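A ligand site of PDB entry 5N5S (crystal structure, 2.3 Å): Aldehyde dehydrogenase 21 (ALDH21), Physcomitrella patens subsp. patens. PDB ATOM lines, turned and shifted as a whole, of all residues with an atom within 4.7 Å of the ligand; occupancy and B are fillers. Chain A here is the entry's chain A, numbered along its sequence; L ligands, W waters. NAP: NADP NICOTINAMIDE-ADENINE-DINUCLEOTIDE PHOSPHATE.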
ATOM      1  N   VAL A 185     -12.251  17.897 -32.019  1.00  0.00           N
ATOM      2  CA  VAL A 185     -13.696  17.673 -31.902  1.00  0.00           C
ATOM      3  C   VAL A 185     -14.121  18.441 -30.636  1.00  0.00           C
ATOM      4  O   VAL A 185     -13.599  18.183 -29.552  1.00  0.00           O
ATOM      5  CB  VAL A 185     -14.073  16.166 -31.870  1.00  0.00           C
ATOM      6  CG1 VAL A 185     -15.584  15.997 -31.827  1.00  0.00           C
ATOM      7  CG2 VAL A 185     -13.490  15.407 -33.061  1.00  0.00           C
ATOM      8  N   SER A 186     -15.017  19.417 -30.807  1.00  0.00           N
ATOM      9  CA  SER A 186     -15.453  20.333 -29.740  1.00  0.00           C
ATOM     10  C   SER A 186     -16.942  20.195 -29.399  1.00  0.00           C
ATOM     11  O   SER A 186     -17.705  19.715 -30.246  1.00  0.00           O
ATOM     12  CB  SER A 186     -15.114  21.768 -30.129  1.00  0.00           C
ATOM     13  OG  SER A 186     -15.622  22.107 -31.409  1.00  0.00           O
ATOM     14  N   PRO A 187     -17.402  20.585 -28.170  1.00  0.00           N
ATOM     15  CA  PRO A 187     -18.836  20.415 -27.831  1.00  0.00           C
ATOM     16  C   PRO A 187     -19.679  21.651 -28.167  1.00  0.00           C
ATOM     17  O   PRO A 187     -19.177  22.591 -28.792  1.00  0.00           O
ATOM     18  CB  PRO A 187     -18.796  20.166 -26.323  1.00  0.00           C
ATOM     19  CG  PRO A 187     -17.609  20.959 -25.852  1.00  0.00           C
ATOM     20  CD  PRO A 187     -16.672  21.165 -27.014  1.00  0.00           C
ATOM     21  N   TRP A 188     -20.944  21.652 -27.755  1.00  0.00           N
ATOM     22  CA  TRP A 188     -21.859  22.748 -28.037  1.00  0.00           C
ATOM     23  C   TRP A 188     -21.837  23.884 -26.994  1.00  0.00           C
ATOM     24  O   TRP A 188     -22.117  25.017 -27.374  1.00  0.00           O
ATOM     25  CB  TRP A 188     -23.322  22.232 -28.268  1.00  0.00           C
ATOM     26  CG  TRP A 188     -24.068  21.863 -27.004  1.00  0.00           C
ATOM     27  CD1 TRP A 188     -24.195  20.616 -26.483  1.00  0.00           C
ATOM     28  CD2 TRP A 188     -24.687  22.766 -26.071  1.00  0.00           C
ATOM     29  NE1 TRP A 188     -24.868  20.671 -25.274  1.00  0.00           N
ATOM     30  CE2 TRP A 188     -25.164  21.984 -24.994  1.00  0.00           C
ATOM     31  CE3 TRP A 188     -24.902  24.150 -26.047  1.00  0.00           C
ATOM     32  CZ2 TRP A 188     -25.823  22.548 -23.901  1.00  0.00           C
ATOM     33  CZ3 TRP A 188     -25.532  24.719 -24.956  1.00  0.00           C
ATOM     34  CH2 TRP A 188     -26.014  23.914 -23.907  1.00  0.00           C
ATOM     35  N   ASN A 189     -21.609  23.576 -25.673  1.00  0.00           N
ATOM     36  CA  ASN A 189     -21.788  24.539 -24.574  1.00  0.00           C
ATOM     37  C   ASN A 189     -20.841  25.749 -24.591  1.00  0.00           C
ATOM     38  O   ASN A 189     -21.284  26.845 -24.231  1.00  0.00           O
ATOM     39  CB  ASN A 189     -21.808  23.893 -23.185  1.00  0.00           C
ATOM     40  CG  ASN A 189     -20.676  22.978 -22.843  1.00  0.00           C
ATOM     41  OD1 ASN A 189     -20.170  22.228 -23.671  1.00  0.00           O
ATOM     42  ND2 ASN A 189     -20.300  22.997 -21.568  1.00  0.00           N
ATOM     43  N   LEU A 194     -13.814  26.714 -26.170  1.00  0.00           N
ATOM     44  CA  LEU A 194     -13.285  25.350 -26.176  1.00  0.00           C
ATOM     45  C   LEU A 194     -12.637  24.981 -27.501  1.00  0.00           C
ATOM     46  O   LEU A 194     -11.771  24.116 -27.539  1.00  0.00           O
ATOM     47  CB  LEU A 194     -14.321  24.320 -25.724  1.00  0.00           C
ATOM     48  CG  LEU A 194     -14.688  24.440 -24.251  1.00  0.00           C
ATOM     49  CD1 LEU A 194     -15.948  23.705 -23.960  1.00  0.00           C
ATOM     50  CD2 LEU A 194     -13.547  24.001 -23.337  1.00  0.00           C
ATOM     51  N   LYS A 212     -13.737  19.668 -36.249  1.00  0.00           N
ATOM     52  CA  LYS A 212     -15.113  19.244 -36.396  1.00  0.00           C
ATOM     53  C   LYS A 212     -15.881  19.846 -35.202  1.00  0.00           C
ATOM     54  O   LYS A 212     -15.879  19.287 -34.108  1.00  0.00           O
ATOM     55  CB  LYS A 212     -15.241  17.718 -36.458  1.00  0.00           C
ATOM     56  CG  LYS A 212     -16.671  17.215 -36.663  1.00  0.00           C
ATOM     57  CD  LYS A 212     -17.107  16.415 -35.434  1.00  0.00           C
ATOM     58  CE  LYS A 212     -18.580  16.162 -35.349  1.00  0.00           C
ATOM     59  NZ  LYS A 212     -19.348  17.391 -35.038  1.00  0.00           N
ATOM     60  N   PRO A 213     -16.500  21.036 -35.388  1.00  0.00           N
ATOM     61  CA  PRO A 213     -17.274  21.623 -34.288  1.00  0.00           C
ATOM     62  C   PRO A 213     -18.626  20.918 -34.141  1.00  0.00           C
ATOM     63  O   PRO A 213     -18.974  20.121 -35.006  1.00  0.00           O
ATOM     64  CB  PRO A 213     -17.424  23.101 -34.692  1.00  0.00           C
ATOM     65  CG  PRO A 213     -17.184  23.147 -36.164  1.00  0.00           C
ATOM     66  CD  PRO A 213     -16.585  21.846 -36.626  1.00  0.00           C
ATOM     67  N   ALA A 214     -19.379  21.196 -33.056  1.00  0.00           N
ATOM     68  CA  ALA A 214     -20.710  20.608 -32.845  1.00  0.00           C
ATOM     69  C   ALA A 214     -21.683  21.165 -33.899  1.00  0.00           C
ATOM     70  O   ALA A 214     -21.688  22.375 -34.145  1.00  0.00           O
ATOM     71  CB  ALA A 214     -21.206  20.917 -31.438  1.00  0.00           C
ATOM     72  N   SER A 215     -22.459  20.270 -34.540  1.00  0.00           N
ATOM     73  CA  SER A 215     -23.444  20.587 -35.581  1.00  0.00           C
ATOM     74  C   SER A 215     -24.450  21.651 -35.167  1.00  0.00           C
ATOM     75  O   SER A 215     -24.811  22.488 -35.998  1.00  0.00           O
ATOM     76  CB  SER A 215     -24.202  19.326 -35.998  1.00  0.00           C
ATOM     77  OG  SER A 215     -23.350  18.433 -36.692  1.00  0.00           O
ATOM     78  N   ARG A 216     -24.900  21.630 -33.908  1.00  0.00           N
ATOM     79  CA  ARG A 216     -25.867  22.577 -33.342  1.00  0.00           C
ATOM     80  C   ARG A 216     -25.274  23.979 -33.158  1.00  0.00           C
ATOM     81  O   ARG A 216     -26.020  24.960 -33.234  1.00  0.00           O
ATOM     82  CB  ARG A 216     -26.430  22.050 -32.023  1.00  0.00           C
ATOM     83  CG  ARG A 216     -27.453  20.916 -32.182  1.00  0.00           C
ATOM     84  CD  ARG A 216     -27.772  20.244 -30.851  1.00  0.00           C
ATOM     85  NE  ARG A 216     -26.637  19.480 -30.322  1.00  0.00           N
ATOM     86  CZ  ARG A 216     -26.598  18.883 -29.139  1.00  0.00           C
ATOM     87  NH1 ARG A 216     -27.654  18.954 -28.322  1.00  0.00           N
ATOM     88  NH2 ARG A 216     -25.522  18.218 -28.751  1.00  0.00           N
ATOM     89  N   VAL A 244     -19.851  18.636 -39.403  1.00  0.00           N
ATOM     90  CA  VAL A 244     -20.551  17.431 -39.859  1.00  0.00           C
ATOM     91  C   VAL A 244     -21.203  16.750 -38.668  1.00  0.00           C
ATOM     92  O   VAL A 244     -20.769  16.967 -37.530  1.00  0.00           O
ATOM     93  CB  VAL A 244     -19.678  16.440 -40.690  1.00  0.00           C
ATOM     94  CG1 VAL A 244     -19.365  16.995 -42.060  1.00  0.00           C
ATOM     95  CG2 VAL A 244     -18.399  16.039 -39.956  1.00  0.00           C
ATOM     96  N   SER A 245     -22.232  15.944 -38.918  1.00  0.00           N
ATOM     97  CA  SER A 245     -22.902  15.204 -37.850  1.00  0.00           C
ATOM     98  C   SER A 245     -22.002  14.050 -37.415  1.00  0.00           C
ATOM     99  O   SER A 245     -21.130  13.613 -38.186  1.00  0.00           O
ATOM    100  CB  SER A 245     -24.261  14.701 -38.322  1.00  0.00           C
ATOM    101  OG  SER A 245     -25.112  14.513 -37.196  1.00  0.00           O
ATOM    102  N   ARG A 246     -22.198  13.561 -36.167  1.00  0.00           N
ATOM    103  CA  ARG A 246     -21.421  12.483 -35.546  1.00  0.00           C
ATOM    104  C   ARG A 246     -21.324  11.172 -36.377  1.00  0.00           C
ATOM    105  O   ARG A 246     -20.318  10.466 -36.272  1.00  0.00           O
ATOM    106  CB  ARG A 246     -21.934  12.203 -34.132  1.00  0.00           C
ATOM    107  CG  ARG A 246     -23.409  11.827 -33.978  1.00  0.00           C
ATOM    108  CD  ARG A 246     -23.779  11.726 -32.513  1.00  0.00           C
ATOM    109  NE  ARG A 246     -23.867  13.040 -31.884  1.00  0.00           N
ATOM    110  CZ  ARG A 246     -23.728  13.278 -30.586  1.00  0.00           C
ATOM    111  NH1 ARG A 246     -23.804  14.513 -30.117  1.00  0.00           N
ATOM    112  NH2 ARG A 246     -23.483  12.279 -29.748  1.00  0.00           N
ATOM    113  N   ALA A 249     -18.442  11.831 -39.034  1.00  0.00           N
ATOM    114  CA  ALA A 249     -17.142  12.222 -38.502  1.00  0.00           C
ATOM    115  C   ALA A 249     -16.292  11.094 -37.905  1.00  0.00           C
ATOM    116  O   ALA A 249     -15.543  11.322 -36.942  1.00  0.00           O
ATOM    117  CB  ALA A 249     -17.334  13.343 -37.488  1.00  0.00           C
ATOM    118  N   THR A 253     -11.564  10.318 -35.766  1.00  0.00           N
ATOM    119  CA  THR A 253     -11.142   9.410 -34.719  1.00  0.00           C
ATOM    120  C   THR A 253     -10.057   8.429 -35.172  1.00  0.00           C
ATOM    121  O   THR A 253      -8.995   8.382 -34.562  1.00  0.00           O
ATOM    122  CB  THR A 253     -12.381   8.661 -34.150  1.00  0.00           C
ATOM    123  OG1 THR A 253     -13.277   9.623 -33.593  1.00  0.00           O
ATOM    124  CG2 THR A 253     -12.026   7.623 -33.100  1.00  0.00           C
ATOM    125  N   PHE A 263     -10.239  15.792 -28.000  1.00  0.00           N
ATOM    126  CA  PHE A 263     -11.687  15.782 -27.878  1.00  0.00           C
ATOM    127  C   PHE A 263     -12.179  16.442 -26.598  1.00  0.00           C
ATOM    128  O   PHE A 263     -11.669  16.179 -25.510  1.00  0.00           O
ATOM    129  CB  PHE A 263     -12.208  14.339 -27.972  1.00  0.00           C
ATOM    130  CG  PHE A 263     -13.689  14.135 -27.732  1.00  0.00           C
ATOM    131  CD1 PHE A 263     -14.607  14.234 -28.765  1.00  0.00           C
ATOM    132  CD2 PHE A 263     -14.170  13.833 -26.457  1.00  0.00           C
ATOM    133  CE1 PHE A 263     -15.981  14.049 -28.544  1.00  0.00           C
ATOM    134  CE2 PHE A 263     -15.538  13.655 -26.232  1.00  0.00           C
ATOM    135  CZ  PHE A 263     -16.438  13.759 -27.277  1.00  0.00           C
ATOM    136  N   THR A 264     -13.245  17.241 -26.752  1.00  0.00           N
ATOM    137  CA  THR A 264     -13.968  17.887 -25.658  1.00  0.00           C
ATOM    138  C   THR A 264     -15.442  17.550 -25.885  1.00  0.00           C
ATOM    139  O   THR A 264     -15.990  17.875 -26.948  1.00  0.00           O
ATOM    140  CB  THR A 264     -13.642  19.397 -25.537  1.00  0.00           C
ATOM    141  OG1 THR A 264     -12.254  19.555 -25.315  1.00  0.00           O
ATOM    142  CG2 THR A 264     -14.346  20.048 -24.377  1.00  0.00           C
ATOM    143  N   GLY A 265     -16.028  16.821 -24.944  1.00  0.00           N
ATOM    144  CA  GLY A 265     -17.421  16.384 -25.013  1.00  0.00           C
ATOM    145  C   GLY A 265     -17.779  15.395 -23.927  1.00  0.00           C
ATOM    146  O   GLY A 265     -17.135  15.367 -22.881  1.00  0.00           O
ATOM    147  N   SER A 266     -18.828  14.600 -24.142  1.00  0.00           N
ATOM    148  CA  SER A 266     -19.317  13.650 -23.129  1.00  0.00           C
ATOM    149  C   SER A 266     -18.385  12.451 -22.948  1.00  0.00           C
ATOM    150  O   SER A 266     -17.739  12.007 -23.901  1.00  0.00           O
ATOM    151  CB  SER A 266     -20.717  13.166 -23.495  1.00  0.00           C
ATOM    152  OG  SER A 266     -20.673  12.304 -24.616  1.00  0.00           O
ATOM    153  N   ILE A 269     -18.835   9.011 -25.232  1.00  0.00           N
ATOM    154  CA  ILE A 269     -18.406   9.279 -26.622  1.00  0.00           C
ATOM    155  C   ILE A 269     -16.872   9.330 -26.693  1.00  0.00           C
ATOM    156  O   ILE A 269     -16.280   8.690 -27.570  1.00  0.00           O
ATOM    157  CB  ILE A 269     -19.086  10.560 -27.194  1.00  0.00           C
ATOM    158  CG1 ILE A 269     -20.641  10.422 -27.321  1.00  0.00           C
ATOM    159  CG2 ILE A 269     -18.440  11.017 -28.513  1.00  0.00           C
ATOM    160  CD1 ILE A 269     -21.227   9.390 -28.320  1.00  0.00           C
ATOM    161  N   MET A 273     -14.027   6.881 -28.444  1.00  0.00           N
ATOM    162  CA  MET A 273     -13.139   7.491 -29.433  1.00  0.00           C
ATOM    163  C   MET A 273     -11.685   7.167 -29.138  1.00  0.00           C
ATOM    164  O   MET A 273     -10.927   6.944 -30.071  1.00  0.00           O
ATOM    165  CB  MET A 273     -13.333   9.008 -29.502  1.00  0.00           C
ATOM    166  CG  MET A 273     -14.409   9.409 -30.474  1.00  0.00           C
ATOM    167  SD  MET A 273     -14.822  11.160 -30.419  1.00  0.00           S
ATOM    168  CE  MET A 273     -13.496  11.846 -31.297  1.00  0.00           C
ATOM    169  N   ARG A 276     -10.984   3.577 -30.296  1.00  0.00           N
ATOM    170  CA  ARG A 276     -10.961   3.419 -31.759  1.00  0.00           C
ATOM    171  C   ARG A 276      -9.895   4.304 -32.462  1.00  0.00           C
ATOM    172  O   ARG A 276      -9.713   4.200 -33.673  1.00  0.00           O
ATOM    173  CB  ARG A 276     -12.356   3.752 -32.318  1.00  0.00           C
ATOM    174  CG  ARG A 276     -13.455   2.734 -32.024  1.00  0.00           C
ATOM    175  CD  ARG A 276     -14.853   3.336 -32.106  1.00  0.00           C
ATOM    176  NE  ARG A 276     -14.989   4.289 -33.213  1.00  0.00           N
ATOM    177  CZ  ARG A 276     -15.365   5.560 -33.070  1.00  0.00           C
ATOM    178  NH1 ARG A 276     -15.659   6.042 -31.876  1.00  0.00           N
ATOM    179  NH2 ARG A 276     -15.439   6.363 -34.130  1.00  0.00           N
ATOM    180  N   GLU A 285     -11.161  15.763 -22.741  1.00  0.00           N
ATOM    181  CA  GLU A 285     -11.784  16.734 -21.847  1.00  0.00           C
ATOM    182  C   GLU A 285     -13.254  16.343 -21.778  1.00  0.00           C
ATOM    183  O   GLU A 285     -14.023  16.642 -22.680  1.00  0.00           O
ATOM    184  CB  GLU A 285     -11.578  18.172 -22.397  1.00  0.00           C
ATOM    185  CG  GLU A 285     -10.179  18.734 -22.199  1.00  0.00           C
ATOM    186  CD  GLU A 285      -9.738  19.011 -20.767  1.00  0.00           C
ATOM    187  OE1 GLU A 285      -8.504  18.990 -20.526  1.00  0.00           O
ATOM    188  OE2 GLU A 285     -10.603  19.229 -19.893  1.00  0.00           O
ATOM    189  N   LEU A 286     -13.628  15.587 -20.726  1.00  0.00           N
ATOM    190  CA  LEU A 286     -14.971  15.008 -20.590  1.00  0.00           C
ATOM    191  C   LEU A 286     -15.829  15.645 -19.475  1.00  0.00           C
ATOM    192  O   LEU A 286     -15.531  16.752 -19.019  1.00  0.00           O
ATOM    193  CB  LEU A 286     -14.840  13.472 -20.465  1.00  0.00           C
ATOM    194  CG  LEU A 286     -13.822  12.833 -21.463  1.00  0.00           C
ATOM    195  CD1 LEU A 286     -13.437  11.494 -21.057  1.00  0.00           C
ATOM    196  CD2 LEU A 286     -14.326  12.832 -22.884  1.00  0.00           C
ATOM    197  N   GLY A 287     -16.932  14.974 -19.130  1.00  0.00           N
ATOM    198  CA  GLY A 287     -17.907  15.451 -18.164  1.00  0.00           C
ATOM    199  C   GLY A 287     -17.472  15.495 -16.715  1.00  0.00           C
ATOM    200  O   GLY A 287     -16.379  15.024 -16.368  1.00  0.00           O
ATOM    201  N   GLY A 288     -18.346  16.038 -15.872  1.00  0.00           N
ATOM    202  CA  GLY A 288     -18.115  16.139 -14.441  1.00  0.00           C
ATOM    203  C   GLY A 288     -19.366  16.191 -13.597  1.00  0.00           C
ATOM    204  O   GLY A 288     -20.445  16.541 -14.084  1.00  0.00           O
ATOM    205  N   CYS A 320     -19.379  21.734 -17.795  1.00  0.00           N
ATOM    206  CA  CYS A 320     -18.589  20.558 -17.382  1.00  0.00           C
ATOM    207  C   CYS A 320     -18.119  20.685 -15.930  1.00  0.00           C
ATOM    208  O   CYS A 320     -17.803  19.670 -15.303  1.00  0.00           O
ATOM    209  CB  CYS A 320     -17.395  20.368 -18.303  1.00  0.00           C
ATOM    210  SG  CYS A 320     -16.471  21.890 -18.671  1.00  0.00           S
ATOM    211  N   GLU A 414     -23.800  12.825 -14.422  1.00  0.00           N
ATOM    212  CA  GLU A 414     -23.691  14.254 -14.673  1.00  0.00           C
ATOM    213  C   GLU A 414     -25.061  14.784 -15.060  1.00  0.00           C
ATOM    214  O   GLU A 414     -25.719  14.234 -15.967  1.00  0.00           O
ATOM    215  CB  GLU A 414     -22.656  14.538 -15.767  1.00  0.00           C
ATOM    216  CG  GLU A 414     -22.589  15.987 -16.224  1.00  0.00           C
ATOM    217  CD  GLU A 414     -21.578  16.259 -17.310  1.00  0.00           C
ATOM    218  OE1 GLU A 414     -21.508  15.452 -18.263  1.00  0.00           O
ATOM    219  OE2 GLU A 414     -20.859  17.289 -17.215  1.00  0.00           O
ATOM    220  N   PHE A 416     -25.928  18.250 -15.963  1.00  0.00           N
ATOM    221  CA  PHE A 416     -25.837  19.183 -17.103  1.00  0.00           C
ATOM    222  C   PHE A 416     -27.178  19.937 -17.266  1.00  0.00           C
ATOM    223  O   PHE A 416     -27.773  19.981 -18.339  1.00  0.00           O
ATOM    224  CB  PHE A 416     -25.356  18.460 -18.382  1.00  0.00           C
ATOM    225  CG  PHE A 416     -24.531  19.299 -19.326  1.00  0.00           C
ATOM    226  CD1 PHE A 416     -23.257  19.712 -18.975  1.00  0.00           C
ATOM    227  CD2 PHE A 416     -25.007  19.616 -20.589  1.00  0.00           C
ATOM    228  CE1 PHE A 416     -22.493  20.483 -19.855  1.00  0.00           C
ATOM    229  CE2 PHE A 416     -24.254  20.394 -21.467  1.00  0.00           C
ATOM    230  CZ  PHE A 416     -22.987  20.817 -21.096  1.00  0.00           C
ATOM    231  N   LEU A 442     -13.346  16.167 -12.348  1.00  0.00           N
ATOM    232  CA  LEU A 442     -12.931  17.362 -13.068  1.00  0.00           C
ATOM    233  C   LEU A 442     -12.440  18.429 -12.087  1.00  0.00           C
ATOM    234  O   LEU A 442     -11.221  18.633 -11.970  1.00  0.00           O
ATOM    235  CB  LEU A 442     -14.043  17.836 -14.041  1.00  0.00           C
ATOM    236  CG  LEU A 442     -13.600  18.635 -15.277  1.00  0.00           C
ATOM    237  CD1 LEU A 442     -12.606  17.868 -16.133  1.00  0.00           C
ATOM    238  CD2 LEU A 442     -14.763  18.973 -16.155  1.00  0.00           C
ATOM    239  N   ARG A 475     -12.604  28.699 -13.771  1.00  0.00           N
ATOM    240  CA  ARG A 475     -11.512  28.321 -14.656  1.00  0.00           C
ATOM    241  C   ARG A 475     -10.794  29.552 -15.188  1.00  0.00           C
ATOM    242  O   ARG A 475     -11.424  30.455 -15.742  1.00  0.00           O
ATOM    243  CB  ARG A 475     -12.003  27.409 -15.816  1.00  0.00           C
ATOM    244  CG  ARG A 475     -10.859  26.887 -16.677  1.00  0.00           C
ATOM    245  CD  ARG A 475     -11.317  26.348 -18.020  1.00  0.00           C
ATOM    246  NE  ARG A 475     -10.183  25.895 -18.835  1.00  0.00           N
ATOM    247  CZ  ARG A 475     -10.290  25.160 -19.928  1.00  0.00           C
ATOM    248  NH1 ARG A 475     -11.472  24.748 -20.348  1.00  0.00           N
ATOM    249  NH2 ARG A 475      -9.201  24.793 -20.597  1.00  0.00           N
ATOM    250  N   TYR A 481      -5.963  22.494 -16.787  1.00  0.00           N
ATOM    251  CA  TYR A 481      -7.374  22.096 -16.668  1.00  0.00           C
ATOM    252  C   TYR A 481      -7.629  20.742 -17.312  1.00  0.00           C
ATOM    253  O   TYR A 481      -7.307  20.532 -18.471  1.00  0.00           O
ATOM    254  CB  TYR A 481      -8.254  23.181 -17.296  1.00  0.00           C
ATOM    255  CG  TYR A 481      -9.738  22.911 -17.243  1.00  0.00           C
ATOM    256  CD1 TYR A 481     -10.496  23.298 -16.139  1.00  0.00           C
ATOM    257  CD2 TYR A 481     -10.398  22.271 -18.294  1.00  0.00           C
ATOM    258  CE1 TYR A 481     -11.876  23.091 -16.102  1.00  0.00           C
ATOM    259  CE2 TYR A 481     -11.768  22.041 -18.258  1.00  0.00           C
ATOM    260  CZ  TYR A 481     -12.512  22.462 -17.161  1.00  0.00           C
ATOM    261  OH  TYR A 481     -13.862  22.251 -17.137  1.00  0.00           O
HETATM  262  PA  NAP L   1     -21.062  15.127 -27.098  1.00  0.00           P
HETATM  263  O1A NAP L   1     -20.169  14.024 -26.665  1.00  0.00           O
HETATM  264  O2A NAP L   1     -22.466  14.666 -27.548  1.00  0.00           O
HETATM  265  O5B NAP L   1     -20.489  15.764 -28.451  1.00  0.00           O
HETATM  266  C5B NAP L   1     -19.230  16.454 -28.528  1.00  0.00           C
HETATM  267  C4B NAP L   1     -18.775  16.445 -29.973  1.00  0.00           C
HETATM  268  O4B NAP L   1     -18.519  15.086 -30.395  1.00  0.00           O
HETATM  269  C3B NAP L   1     -19.767  17.035 -30.982  1.00  0.00           C
HETATM  270  O3B NAP L   1     -19.055  17.848 -31.911  1.00  0.00           O
HETATM  271  C2B NAP L   1     -20.367  15.790 -31.650  1.00  0.00           C
HETATM  272  O2B NAP L   1     -20.927  16.009 -32.967  1.00  0.00           O
HETATM  273  C1B NAP L   1     -19.180  14.844 -31.623  1.00  0.00           C
HETATM  274  N9A NAP L   1     -19.420  13.406 -31.748  1.00  0.00           N
HETATM  275  C8A NAP L   1     -20.348  12.650 -31.081  1.00  0.00           C
HETATM  276  N7A NAP L   1     -20.283  11.369 -31.345  1.00  0.00           N
HETATM  277  C5A NAP L   1     -19.234  11.270 -32.255  1.00  0.00           C
HETATM  278  C6A NAP L   1     -18.658  10.172 -32.923  1.00  0.00           C
HETATM  279  N6A NAP L   1     -19.115   8.918 -32.837  1.00  0.00           N
HETATM  280  N1A NAP L   1     -17.605  10.415 -33.737  1.00  0.00           N
HETATM  281  C2A NAP L   1     -17.172  11.680 -33.883  1.00  0.00           C
HETATM  282  N3A NAP L   1     -17.647  12.789 -33.316  1.00  0.00           N
HETATM  283  C4A NAP L   1     -18.685  12.517 -32.499  1.00  0.00           C
HETATM  284  O3  NAP L   1     -21.189  16.427 -26.174  1.00  0.00           O
HETATM  285  PN  NAP L   1     -22.007  17.814 -26.148  1.00  0.00           P
HETATM  286  O1N NAP L   1     -23.387  17.552 -25.674  1.00  0.00           O
HETATM  287  O2N NAP L   1     -21.817  18.528 -27.433  1.00  0.00           O
HETATM  288  O5D NAP L   1     -21.262  18.621 -24.987  1.00  0.00           O
HETATM  289  C5D NAP L   1     -21.607  18.491 -23.588  1.00  0.00           C
HETATM  290  C4D NAP L   1     -20.690  17.508 -22.893  1.00  0.00           C
HETATM  291  O4D NAP L   1     -19.318  17.960 -22.999  1.00  0.00           O
HETATM  292  C3D NAP L   1     -20.928  17.336 -21.401  1.00  0.00           C
HETATM  293  O3D NAP L   1     -20.764  15.969 -21.015  1.00  0.00           O
HETATM  294  C2D NAP L   1     -19.869  18.264 -20.794  1.00  0.00           C
HETATM  295  O2D NAP L   1     -19.395  17.957 -19.496  1.00  0.00           O
HETATM  296  C1D NAP L   1     -18.678  17.993 -21.745  1.00  0.00           C
HETATM  297  N1N NAP L   1     -17.742  19.180 -21.704  1.00  0.00           N
HETATM  298  C2N NAP L   1     -16.425  18.989 -21.229  1.00  0.00           C
HETATM  299  C3N NAP L   1     -15.576  20.081 -21.114  1.00  0.00           C
HETATM  300  C7N NAP L   1     -14.210  19.992 -20.485  1.00  0.00           C
HETATM  301  O7N NAP L   1     -13.436  20.935 -20.604  1.00  0.00           O
HETATM  302  N7N NAP L   1     -13.870  18.873 -19.888  1.00  0.00           N
HETATM  303  C4N NAP L   1     -16.056  21.338 -21.482  1.00  0.00           C
HETATM  304  C5N NAP L   1     -17.359  21.494 -21.941  1.00  0.00           C
HETATM  305  C6N NAP L   1     -18.180  20.392 -22.057  1.00  0.00           C
HETATM  306  P2B NAP L   1     -22.410  16.529 -33.236  1.00  0.00           P
HETATM  307  O1X NAP L   1     -22.929  17.562 -32.280  1.00  0.00           O
HETATM  308  O2X NAP L   1     -23.233  15.275 -33.305  1.00  0.00           O
HETATM  309  O3X NAP L   1     -22.252  17.065 -34.639  1.00  0.00           O
HETATM  310  O   HOH W   1     -25.619  15.889 -27.216  1.00  0.00           O
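OG of Ser 215 lies within hydrogen-bond range of O of Val 244, at 3.1 Å.
OE2 of Glu 414 is in hydrogen-bond range of N of Gly 288.
N of Ser 186 sits at hydrogen-bond distance from O of Lys 212.
OH of Tyr 481 sits at hydrogen-bond distance from SG of Cys 320, 3.0 Å away.
NZ of Lys 212 lies within hydrogen-bond range of O of Val 244 (2.9 Å).
The backbone NH of Gly 265 lies within hydrogen-bond range of the backbone carbonyl oxygen of Glu 285, at 3.0 Å.
The backbone carbonyl oxygen (O) of Phe 263 sits at hydrogen-bond distance from the backbone NH (N) of Glu 285.
N of Thr 264 sits at hydrogen-bond distance from O of Val 185, 3.0 Å away.
O3X of the ligand lies close to O of Val 244 (3.3 Å).
The backbone carbonyl oxygen (O) of Gly 265 lies close to an oxygen (O4D) of the ligand, 3.4 Å away.
CG1 of Val 185 touches O4B of the ligand (3.4 Å).
Pro 187 touches the ligand (CB to O5D, 3.2 Å).
Asn 189 touches the ligand (OD1 to C6N, 3.2 Å).
Leu 194 touches the ligand (CD1 to C5N, 3.3 Å).
C of Pro 213 touches O3B of the ligand, 3.8 Å away.
CA of Ala 214 touches O3B of the ligand, at 3.4 Å.
Ser 245 touches the ligand.
O of Ala 249 touches C2A of the ligand (3.5 Å).
Phe 263 touches the ligand (CE1 to O4B, 3.3 Å).
Thr 264 touches the ligand.
Ile 269 touches the ligand.
Gly 287 touches the ligand (CA to O2D, 3.2 Å).
Phe 416 touches the ligand (CE1 to C2D, 3.6 Å).
Leu 442 touches the ligand (CD2 to N7N, 3.8 Å).
CE2 of Tyr 481 touches O7N of the ligand (3.1 Å).
Hydrophobic or aromatic side chains that line the ligand: Val 185, Pro 187, Trp 188, Leu 194, Ala 214, Ala 249, Phe 263, Ile 269, Phe 416, Leu 442 and Tyr 481.
28 residues have an atom within 4 Å of the ligand: Val 185, Ser 186, Pro 187, Trp 188, Asn 189, Leu 194, Lys 212, Pro 213, Ala 214, Ser 215, Arg 216, Val 244, Ser 245, Arg 246, Ala 249, Phe 263, Thr 264, Gly 265, Ser 266, Ile 269, Glu 285, Leu 286, Gly 287, Cys 320, Glu 414, Phe 416, Leu 442 and Tyr 481.
The nearest printed residue that does not touch the ligand is Met 273 (4.2 Å).
N of Ser 215 lies within hydrogen-bond range of O3X of the ligand, 3.2 Å away.
An oxygen (O3X) of the ligand is in hydrogen-bond range of the side-chain hydroxyl of Ser 215, 2.7 Å away.
N of Ser 266 sits at hydrogen-bond distance from O1A of the ligand (2.9 Å).
An oxygen (O1A) of the ligand lies within hydrogen-bond range of the side-chain hydroxyl of Ser 266, at 2.7 Å.
The backbone NH of Arg 246 sits close to an oxygen (O2X) of the ligand (3.5 Å).
An oxygen (O2X) of the ligand is in salt-bridge range of the guanidinium group (NE) of Arg 246, at 2.7 Å.
OE2 of Glu 414 is in hydrogen-bond range of O2D of the ligand, 2.8 Å away.
The backbone carbonyl oxygen (O) of Leu 286 is in hydrogen-bond range of a nitrogen (N7N) of the ligand (2.8 Å).
O3B of the ligand lies within hydrogen-bond range of O of Ser 186, 2.8 Å away.
SG of Cys 320 lies close to O7N of the ligand (3.7 Å).
An oxygen (O3X) of the ligand lies within salt-bridge range of the side-chain amino group of Lys 212, at 2.9 Å.
A nitrogen (N7N) of the ligand lies close to the side-chain carboxylate of Glu 285 (3.3 Å).
An oxygen (O2N) of the ligand lies within hydrogen-bond range of the backbone NH (N) of Trp 188.
An oxygen (O1N) of the ligand lies close to the indole nitrogen (NE1) of Trp 188 (3.5 Å).
The guanidinium group of Arg 216 lies within salt-bridge range of an oxygen (O1N) of the ligand, at 3.8 Å.
Water W1 lies within hydrogen-bond range of the guanidinium group of Arg 216 and an oxygen (O1N) of the ligand.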
